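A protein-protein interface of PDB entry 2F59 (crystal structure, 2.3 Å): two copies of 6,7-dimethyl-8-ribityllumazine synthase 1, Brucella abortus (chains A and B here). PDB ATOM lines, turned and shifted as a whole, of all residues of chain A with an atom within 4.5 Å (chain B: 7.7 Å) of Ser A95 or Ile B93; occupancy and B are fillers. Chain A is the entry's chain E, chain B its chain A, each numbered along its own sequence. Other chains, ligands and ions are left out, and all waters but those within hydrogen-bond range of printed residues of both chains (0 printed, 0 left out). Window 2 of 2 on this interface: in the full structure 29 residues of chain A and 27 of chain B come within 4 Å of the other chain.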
ATOM      1  N   VAL A  83      -4.991 -13.947  19.569  1.00  0.00           N
ATOM      2  CA  VAL A  83      -3.546 -13.938  19.658  1.00  0.00           C
ATOM      3  C   VAL A  83      -3.178 -15.301  20.237  1.00  0.00           C
ATOM      4  O   VAL A  83      -3.652 -15.687  21.314  1.00  0.00           O
ATOM      5  CB  VAL A  83      -3.043 -12.814  20.589  1.00  0.00           C
ATOM      6  CG1 VAL A  83      -1.532 -12.856  20.677  1.00  0.00           C
ATOM      7  CG2 VAL A  83      -3.503 -11.457  20.073  1.00  0.00           C
ATOM      8  N   PHE A  91       3.835 -12.138  20.111  1.00  0.00           N
ATOM      9  CA  PHE A  91       2.434 -12.396  20.420  1.00  0.00           C
ATOM     10  C   PHE A  91       1.962 -11.744  21.724  1.00  0.00           C
ATOM     11  O   PHE A  91       0.854 -11.209  21.792  1.00  0.00           O
ATOM     12  CB  PHE A  91       2.179 -13.907  20.472  1.00  0.00           C
ATOM     13  CG  PHE A  91       2.644 -14.644  19.246  1.00  0.00           C
ATOM     14  CD1 PHE A  91       3.981 -14.991  19.093  1.00  0.00           C
ATOM     15  CD2 PHE A  91       1.749 -14.986  18.238  1.00  0.00           C
ATOM     16  CE1 PHE A  91       4.423 -15.669  17.959  1.00  0.00           C
ATOM     17  CE2 PHE A  91       2.179 -15.664  17.098  1.00  0.00           C
ATOM     18  CZ  PHE A  91       3.520 -16.006  16.959  1.00  0.00           C
ATOM     19  N   ASP A  92       2.805 -11.782  22.753  1.00  0.00           N
ATOM     20  CA  ASP A  92       2.456 -11.204  24.049  1.00  0.00           C
ATOM     21  C   ASP A  92       2.212  -9.697  23.956  1.00  0.00           C
ATOM     22  O   ASP A  92       1.346  -9.161  24.644  1.00  0.00           O
ATOM     23  CB  ASP A  92       3.566 -11.497  25.065  1.00  0.00           C
ATOM     24  CG  ASP A  92       3.188 -11.092  26.479  1.00  0.00           C
ATOM     25  OD1 ASP A  92       2.118 -11.523  26.956  1.00  0.00           O
ATOM     26  OD2 ASP A  92       3.964 -10.347  27.116  1.00  0.00           O
ATOM     27  N   ILE A  93       2.971  -9.022  23.100  1.00  0.00           N
ATOM     28  CA  ILE A  93       2.824  -7.580  22.917  1.00  0.00           C
ATOM     29  C   ILE A  93       1.477  -7.207  22.295  1.00  0.00           C
ATOM     30  O   ILE A  93       0.829  -6.250  22.726  1.00  0.00           O
ATOM     31  CB  ILE A  93       3.954  -7.019  22.025  1.00  0.00           C
ATOM     32  CG1 ILE A  93       5.273  -7.032  22.799  1.00  0.00           C
ATOM     33  CG2 ILE A  93       3.604  -5.608  21.543  1.00  0.00           C
ATOM     34  CD1 ILE A  93       6.416  -6.390  22.053  1.00  0.00           C
ATOM     35  N   VAL A  94       1.062  -7.958  21.280  1.00  0.00           N
ATOM     36  CA  VAL A  94      -0.206  -7.689  20.613  1.00  0.00           C
ATOM     37  C   VAL A  94      -1.362  -7.714  21.609  1.00  0.00           C
ATOM     38  O   VAL A  94      -2.236  -6.846  21.585  1.00  0.00           O
ATOM     39  CB  VAL A  94      -0.487  -8.719  19.497  1.00  0.00           C
ATOM     40  CG1 VAL A  94      -1.824  -8.417  18.824  1.00  0.00           C
ATOM     41  CG2 VAL A  94       0.638  -8.691  18.478  1.00  0.00           C
ATOM     42  N   SER A  95      -1.357  -8.709  22.487  1.00  0.00           N
ATOM     43  CA  SER A  95      -2.405  -8.839  23.490  1.00  0.00           C
ATOM     44  C   SER A  95      -2.380  -7.694  24.496  1.00  0.00           C
ATOM     45  O   SER A  95      -3.402  -7.053  24.735  1.00  0.00           O
ATOM     46  CB  SER A  95      -2.272 -10.170  24.231  1.00  0.00           C
ATOM     47  OG  SER A  95      -2.607 -11.255  23.384  1.00  0.00           O
ATOM     48  N   ASN A  96      -1.208  -7.439  25.075  1.00  0.00           N
ATOM     49  CA  ASN A  96      -1.058  -6.381  26.069  1.00  0.00           C
ATOM     50  C   ASN A  96      -1.462  -5.006  25.574  1.00  0.00           C
ATOM     51  O   ASN A  96      -2.247  -4.321  26.222  1.00  0.00           O
ATOM     52  CB  ASN A  96       0.385  -6.305  26.578  1.00  0.00           C
ATOM     53  CG  ASN A  96       0.767  -7.500  27.422  1.00  0.00           C
ATOM     54  OD1 ASN A  96      -0.073  -8.085  28.102  1.00  0.00           O
ATOM     55  ND2 ASN A  96       2.048  -7.859  27.396  1.00  0.00           N
ATOM     56  N   GLU A  97      -0.914  -4.602  24.434  1.00  0.00           N
ATOM     57  CA  GLU A  97      -1.211  -3.295  23.877  1.00  0.00           C
ATOM     58  C   GLU A  97      -2.668  -3.093  23.487  1.00  0.00           C
ATOM     59  O   GLU A  97      -3.311  -2.146  23.942  1.00  0.00           O
ATOM     60  CB  GLU A  97      -0.291  -3.026  22.688  1.00  0.00           C
ATOM     61  CG  GLU A  97       1.116  -2.712  23.133  1.00  0.00           C
ATOM     62  CD  GLU A  97       1.112  -1.734  24.294  1.00  0.00           C
ATOM     63  OE1 GLU A  97       1.459  -2.140  25.432  1.00  0.00           O
ATOM     64  OE2 GLU A  97       0.735  -0.563  24.068  1.00  0.00           O
ATOM     65  N   SER A  98      -3.198  -3.979  22.655  1.00  0.00           N
ATOM     66  CA  SER A  98      -4.584  -3.854  22.244  1.00  0.00           C
ATOM     67  C   SER A  98      -5.495  -3.685  23.461  1.00  0.00           C
ATOM     68  O   SER A  98      -6.245  -2.712  23.556  1.00  0.00           O
ATOM     69  CB  SER A  98      -5.017  -5.081  21.427  1.00  0.00           C
ATOM     70  OG  SER A  98      -4.831  -6.292  22.146  1.00  0.00           O
ATOM     71  N   CYS A  99      -5.411  -4.617  24.406  1.00  0.00           N
ATOM     72  CA  CYS A  99      -6.254  -4.568  25.597  1.00  0.00           C
ATOM     73  C   CYS A  99      -5.933  -3.392  26.516  1.00  0.00           C
ATOM     74  O   CYS A  99      -6.813  -2.844  27.181  1.00  0.00           O
ATOM     75  CB  CYS A  99      -6.149  -5.894  26.345  1.00  0.00           C
ATOM     76  SG  CYS A  99      -6.616  -7.286  25.273  1.00  0.00           S
ATOM     77  N   THR A 119      -6.580 -14.271  23.798  1.00  0.00           N
ATOM     78  CA  THR A 119      -5.145 -14.504  23.899  1.00  0.00           C
ATOM     79  C   THR A 119      -4.973 -15.891  24.482  1.00  0.00           C
ATOM     80  O   THR A 119      -5.130 -16.081  25.687  1.00  0.00           O
ATOM     81  CB  THR A 119      -4.461 -13.514  24.851  1.00  0.00           C
ATOM     82  OG1 THR A 119      -4.777 -12.172  24.464  1.00  0.00           O
ATOM     83  CG2 THR A 119      -2.953 -13.717  24.812  1.00  0.00           C
ATOM     84  N   ALA B  53     -13.149  -7.958  35.135  1.00  0.00           N
ATOM     85  CA  ALA B  53     -12.299  -6.908  35.673  1.00  0.00           C
ATOM     86  C   ALA B  53     -11.962  -5.850  34.632  1.00  0.00           C
ATOM     87  O   ALA B  53     -11.764  -4.683  34.977  1.00  0.00           O
ATOM     88  CB  ALA B  53     -11.022  -7.511  36.241  1.00  0.00           C
ATOM     89  N   LEU B  54     -11.899  -6.246  33.363  1.00  0.00           N
ATOM     90  CA  LEU B  54     -11.585  -5.281  32.315  1.00  0.00           C
ATOM     91  C   LEU B  54     -12.569  -4.116  32.253  1.00  0.00           C
ATOM     92  O   LEU B  54     -12.187  -3.016  31.864  1.00  0.00           O
ATOM     93  CB  LEU B  54     -11.497  -5.957  30.942  1.00  0.00           C
ATOM     94  CG  LEU B  54     -10.198  -6.726  30.675  1.00  0.00           C
ATOM     95  CD1 LEU B  54     -10.173  -7.234  29.240  1.00  0.00           C
ATOM     96  CD2 LEU B  54      -9.012  -5.822  30.933  1.00  0.00           C
ATOM     97  N   VAL B  83      -8.940 -12.811  39.104  1.00  0.00           N
ATOM     98  CA  VAL B  83      -8.323 -13.342  37.905  1.00  0.00           C
ATOM     99  C   VAL B  83      -7.404 -14.465  38.376  1.00  0.00           C
ATOM    100  O   VAL B  83      -6.505 -14.245  39.187  1.00  0.00           O
ATOM    101  CB  VAL B  83      -7.477 -12.272  37.174  1.00  0.00           C
ATOM    102  CG1 VAL B  83      -6.787 -12.891  35.973  1.00  0.00           C
ATOM    103  CG2 VAL B  83      -8.355 -11.120  36.738  1.00  0.00           C
ATOM    104  N   TYR B  89      -3.019 -17.393  28.255  1.00  0.00           N
ATOM    105  CA  TYR B  89      -2.298 -16.150  28.513  1.00  0.00           C
ATOM    106  C   TYR B  89      -3.281 -14.997  28.690  1.00  0.00           C
ATOM    107  O   TYR B  89      -2.884 -13.837  28.812  1.00  0.00           O
ATOM    108  CB  TYR B  89      -1.355 -15.843  27.344  1.00  0.00           C
ATOM    109  CG  TYR B  89       0.087 -15.640  27.748  1.00  0.00           C
ATOM    110  CD1 TYR B  89       0.831 -16.684  28.300  1.00  0.00           C
ATOM    111  CD2 TYR B  89       0.708 -14.402  27.589  1.00  0.00           C
ATOM    112  CE1 TYR B  89       2.158 -16.499  28.682  1.00  0.00           C
ATOM    113  CE2 TYR B  89       2.035 -14.208  27.968  1.00  0.00           C
ATOM    114  CZ  TYR B  89       2.752 -15.259  28.513  1.00  0.00           C
ATOM    115  OH  TYR B  89       4.062 -15.070  28.886  1.00  0.00           O
ATOM    116  N   HIS B  90      -4.567 -15.332  28.713  1.00  0.00           N
ATOM    117  CA  HIS B  90      -5.633 -14.344  28.847  1.00  0.00           C
ATOM    118  C   HIS B  90      -5.989 -14.062  30.309  1.00  0.00           C
ATOM    119  O   HIS B  90      -7.161 -13.892  30.645  1.00  0.00           O
ATOM    120  CB  HIS B  90      -6.872 -14.842  28.087  1.00  0.00           C
ATOM    121  CG  HIS B  90      -7.924 -13.797  27.873  1.00  0.00           C
ATOM    122  ND1 HIS B  90      -8.658 -13.252  28.904  1.00  0.00           N
ATOM    123  CD2 HIS B  90      -8.366 -13.199  26.740  1.00  0.00           C
ATOM    124  CE1 HIS B  90      -9.506 -12.364  28.419  1.00  0.00           C
ATOM    125  NE2 HIS B  90      -9.349 -12.312  27.108  1.00  0.00           N
ATOM    126  N   PHE B  91      -4.987 -14.001  31.182  1.00  0.00           N
ATOM    127  CA  PHE B  91      -5.266 -13.745  32.591  1.00  0.00           C
ATOM    128  C   PHE B  91      -4.470 -12.593  33.216  1.00  0.00           C
ATOM    129  O   PHE B  91      -5.049 -11.683  33.813  1.00  0.00           O
ATOM    130  CB  PHE B  91      -5.054 -15.025  33.406  1.00  0.00           C
ATOM    131  CG  PHE B  91      -5.868 -16.199  32.921  1.00  0.00           C
ATOM    132  CD1 PHE B  91      -5.344 -17.091  31.991  1.00  0.00           C
ATOM    133  CD2 PHE B  91      -7.160 -16.411  33.395  1.00  0.00           C
ATOM    134  CE1 PHE B  91      -6.096 -18.178  31.541  1.00  0.00           C
ATOM    135  CE2 PHE B  91      -7.919 -17.497  32.950  1.00  0.00           C
ATOM    136  CZ  PHE B  91      -7.384 -18.380  32.022  1.00  0.00           C
ATOM    137  N   ASP B  92      -3.149 -12.633  33.088  1.00  0.00           N
ATOM    138  CA  ASP B  92      -2.304 -11.585  33.650  1.00  0.00           C
ATOM    139  C   ASP B  92      -2.617 -10.244  32.996  1.00  0.00           C
ATOM    140  O   ASP B  92      -2.360  -9.184  33.570  1.00  0.00           O
ATOM    141  CB  ASP B  92      -0.824 -11.929  33.453  1.00  0.00           C
ATOM    142  CG  ASP B  92      -0.428 -13.220  34.144  1.00  0.00           C
ATOM    143  OD1 ASP B  92      -0.674 -13.343  35.364  1.00  0.00           O
ATOM    144  OD2 ASP B  92       0.134 -14.110  33.471  1.00  0.00           O
ATOM    145  N   ILE B  93      -3.169 -10.294  31.788  1.00  0.00           N
ATOM    146  CA  ILE B  93      -3.530  -9.082  31.070  1.00  0.00           C
ATOM    147  C   ILE B  93      -4.717  -8.404  31.752  1.00  0.00           C
ATOM    148  O   ILE B  93      -4.719  -7.187  31.946  1.00  0.00           O
ATOM    149  CB  ILE B  93      -3.898  -9.391  29.602  1.00  0.00           C
ATOM    150  CG1 ILE B  93      -2.629  -9.716  28.814  1.00  0.00           C
ATOM    151  CG2 ILE B  93      -4.632  -8.212  28.979  1.00  0.00           C
ATOM    152  CD1 ILE B  93      -2.886 -10.077  27.375  1.00  0.00           C
ATOM    153  N   VAL B  94      -5.721  -9.197  32.115  1.00  0.00           N
ATOM    154  CA  VAL B  94      -6.907  -8.667  32.770  1.00  0.00           C
ATOM    155  C   VAL B  94      -6.543  -7.934  34.060  1.00  0.00           C
ATOM    156  O   VAL B  94      -6.966  -6.798  34.278  1.00  0.00           O
ATOM    157  CB  VAL B  94      -7.925  -9.790  33.086  1.00  0.00           C
ATOM    158  CG1 VAL B  94      -9.072  -9.237  33.925  1.00  0.00           C
ATOM    159  CG2 VAL B  94      -8.462 -10.384  31.785  1.00  0.00           C
ATOM    160  N   SER B  95      -5.750  -8.579  34.911  1.00  0.00           N
ATOM    161  CA  SER B  95      -5.354  -7.954  36.165  1.00  0.00           C
ATOM    162  C   SER B  95      -4.464  -6.729  35.931  1.00  0.00           C
ATOM    163  O   SER B  95      -4.685  -5.672  36.522  1.00  0.00           O
ATOM    164  CB  SER B  95      -4.632  -8.967  37.060  1.00  0.00           C
ATOM    165  OG  SER B  95      -3.450  -9.457  36.451  1.00  0.00           O
ATOM    166  N   ASN B  96      -3.465  -6.871  35.067  1.00  0.00           N
ATOM    167  CA  ASN B  96      -2.561  -5.766  34.777  1.00  0.00           C
ATOM    168  C   ASN B  96      -3.283  -4.531  34.276  1.00  0.00           C
ATOM    169  O   ASN B  96      -3.101  -3.435  34.805  1.00  0.00           O
ATOM    170  CB  ASN B  96      -1.520  -6.164  33.728  1.00  0.00           C
ATOM    171  CG  ASN B  96      -0.366  -6.936  34.316  1.00  0.00           C
ATOM    172  OD1 ASN B  96      -0.209  -7.009  35.537  1.00  0.00           O
ATOM    173  ND2 ASN B  96       0.462  -7.513  33.447  1.00  0.00           N
ATOM    174  N   GLU B  97      -4.101  -4.712  33.247  1.00  0.00           N
ATOM    175  CA  GLU B  97      -4.814  -3.589  32.665  1.00  0.00           C
ATOM    176  C   GLU B  97      -5.901  -3.027  33.566  1.00  0.00           C
ATOM    177  O   GLU B  97      -6.051  -1.809  33.666  1.00  0.00           O
ATOM    178  CB  GLU B  97      -5.355  -3.982  31.288  1.00  0.00           C
ATOM    179  CG  GLU B  97      -4.222  -4.345  30.334  1.00  0.00           C
ATOM    180  CD  GLU B  97      -3.044  -3.366  30.431  1.00  0.00           C
ATOM    181  OE1 GLU B  97      -1.878  -3.820  30.383  1.00  0.00           O
ATOM    182  OE2 GLU B  97      -3.275  -2.144  30.552  1.00  0.00           O
ATOM    183  N   SER B  98      -6.645  -3.899  34.237  1.00  0.00           N
ATOM    184  CA  SER B  98      -7.679  -3.419  35.140  1.00  0.00           C
ATOM    185  C   SER B  98      -7.009  -2.603  36.249  1.00  0.00           C
ATOM    186  O   SER B  98      -7.406  -1.473  36.516  1.00  0.00           O
ATOM    187  CB  SER B  98      -8.460  -4.592  35.746  1.00  0.00           C
ATOM    188  OG  SER B  98      -7.617  -5.434  36.517  1.00  0.00           O
ATOM    189  N   CYS B  99      -5.983  -3.164  36.884  1.00  0.00           N
ATOM    190  CA  CYS B  99      -5.293  -2.450  37.960  1.00  0.00           C
ATOM    191  C   CYS B  99      -4.584  -1.204  37.446  1.00  0.00           C
ATOM    192  O   CYS B  99      -4.576  -0.164  38.108  1.00  0.00           O
ATOM    193  CB  CYS B  99      -4.273  -3.360  38.653  1.00  0.00           C
ATOM    194  SG  CYS B  99      -4.994  -4.806  39.476  1.00  0.00           S
ATOM    195  N   ARG B 100      -3.980  -1.316  36.268  1.00  0.00           N
ATOM    196  CA  ARG B 100      -3.267  -0.197  35.666  1.00  0.00           C
ATOM    197  C   ARG B 100      -4.202   0.999  35.537  1.00  0.00           C
ATOM    198  O   ARG B 100      -3.894   2.106  35.990  1.00  0.00           O
ATOM    199  CB  ARG B 100      -2.758  -0.576  34.275  1.00  0.00           C
ATOM    200  CG  ARG B 100      -1.728   0.385  33.700  1.00  0.00           C
ATOM    201  CD  ARG B 100      -1.777   0.417  32.169  1.00  0.00           C
ATOM    202  NE  ARG B 100      -2.724   1.435  31.711  1.00  0.00           N
ATOM    203  CZ  ARG B 100      -3.969   1.202  31.295  1.00  0.00           C
ATOM    204  NH1 ARG B 100      -4.460  -0.036  31.248  1.00  0.00           N
ATOM    205  NH2 ARG B 100      -4.743   2.227  30.960  1.00  0.00           N
ATOM    206  N   THR B 119      -5.653 -11.097  41.902  1.00  0.00           N
ATOM    207  CA  THR B 119      -4.928 -11.762  40.833  1.00  0.00           C
ATOM    208  C   THR B 119      -4.186 -12.920  41.484  1.00  0.00           C
ATOM    209  O   THR B 119      -3.228 -12.708  42.224  1.00  0.00           O
ATOM    210  CB  THR B 119      -3.895 -10.829  40.185  1.00  0.00           C
ATOM    211  OG1 THR B 119      -4.514  -9.571  39.880  1.00  0.00           O
ATOM    212  CG2 THR B 119      -3.362 -11.455  38.902  1.00  0.00           C
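The backbone NH of His B90 is in hydrogen-bond range of the backbone carbonyl oxygen of Thr A119.
O of Asp A92 sits at hydrogen-bond distance from ND2 of Asn A96. OG of Ser A95 lies within hydrogen-bond range of OG1 of Thr A119 (2.6 Å). The side-chain hydroxyl (OG) of Ser A98 lies within hydrogen-bond range of the side-chain sulfur (SG) of Cys A99 (3.7 Å). The backbone carbonyl oxygen (O) of Ser A95 lies within hydrogen-bond range of the side-chain hydroxyl (OG) of Ser A98. SG of Cys A99 sits at hydrogen-bond distance from O of Ser A95 (3.3 Å).
Among the printed residues, merely in contact across the chains: Asp A92 with Tyr B89 (2.9 Å), Asn A96 with Ile B93 (3.1 Å), Ser A95 with Ile B93 (3.2 Å), Thr A119 with Tyr B89 (3.6 Å) and Cys A99 with Ile B93 (3.8 Å).
Phe A91 touches none of the printed residues of chain B. Printed residues of chain B within 4 Å of Ser A95: Ile B93. Of the printed residues of chain B, Cys A99 touches Ile B93. Of the printed residues of chain B, Thr A119 touches Tyr B89 (3.6 Å) and His B90 (3.2 Å). Printed residues of chain A within 4 Å of Tyr B89: Asp A92 (2.9 Å) and Thr A119 (3.6 Å). Asp B92 touches none of the printed residues of chain A. Of the printed residues of chain A, Ile B93 touches Ser A95 (3.2 Å), Asn A96 (3.1 Å) and Cys A99 (3.8 Å). The nearest residue of chain B that does not touch Ser A95 is Tyr B89 (5.9 Å). The nearest printed residue of chain B that does not touch Asn A96 is Glu B97 (4.2 Å).
Hydrophobic or aromatic side chains of chain B within 4 Å of the printed part of chain A: Tyr B89, His B90 and Ile B93. Among the printed residues, 6 pairs touch across the chains. Among the printed residues, no Asp or Glu carboxylate lies within 4 Å of a Lys or Arg side-chain nitrogen of the other chain.
Ser A95 touches Ile B93, but with the chains exchanged Ile A93 does not touch Ser B95 (14.0 Å). Asn A96 touches Ile B93, but with the chains exchanged Ile A93 does not touch Asn B96 (10.8 Å). Cys A99 touches Ile B93, but with the chains exchanged Ile A93 does not touch Cys B99 (16.0 Å). Of the 6 pairs that touch across the chains among the printed residues, none has its exchanged pair printed and touching as well.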
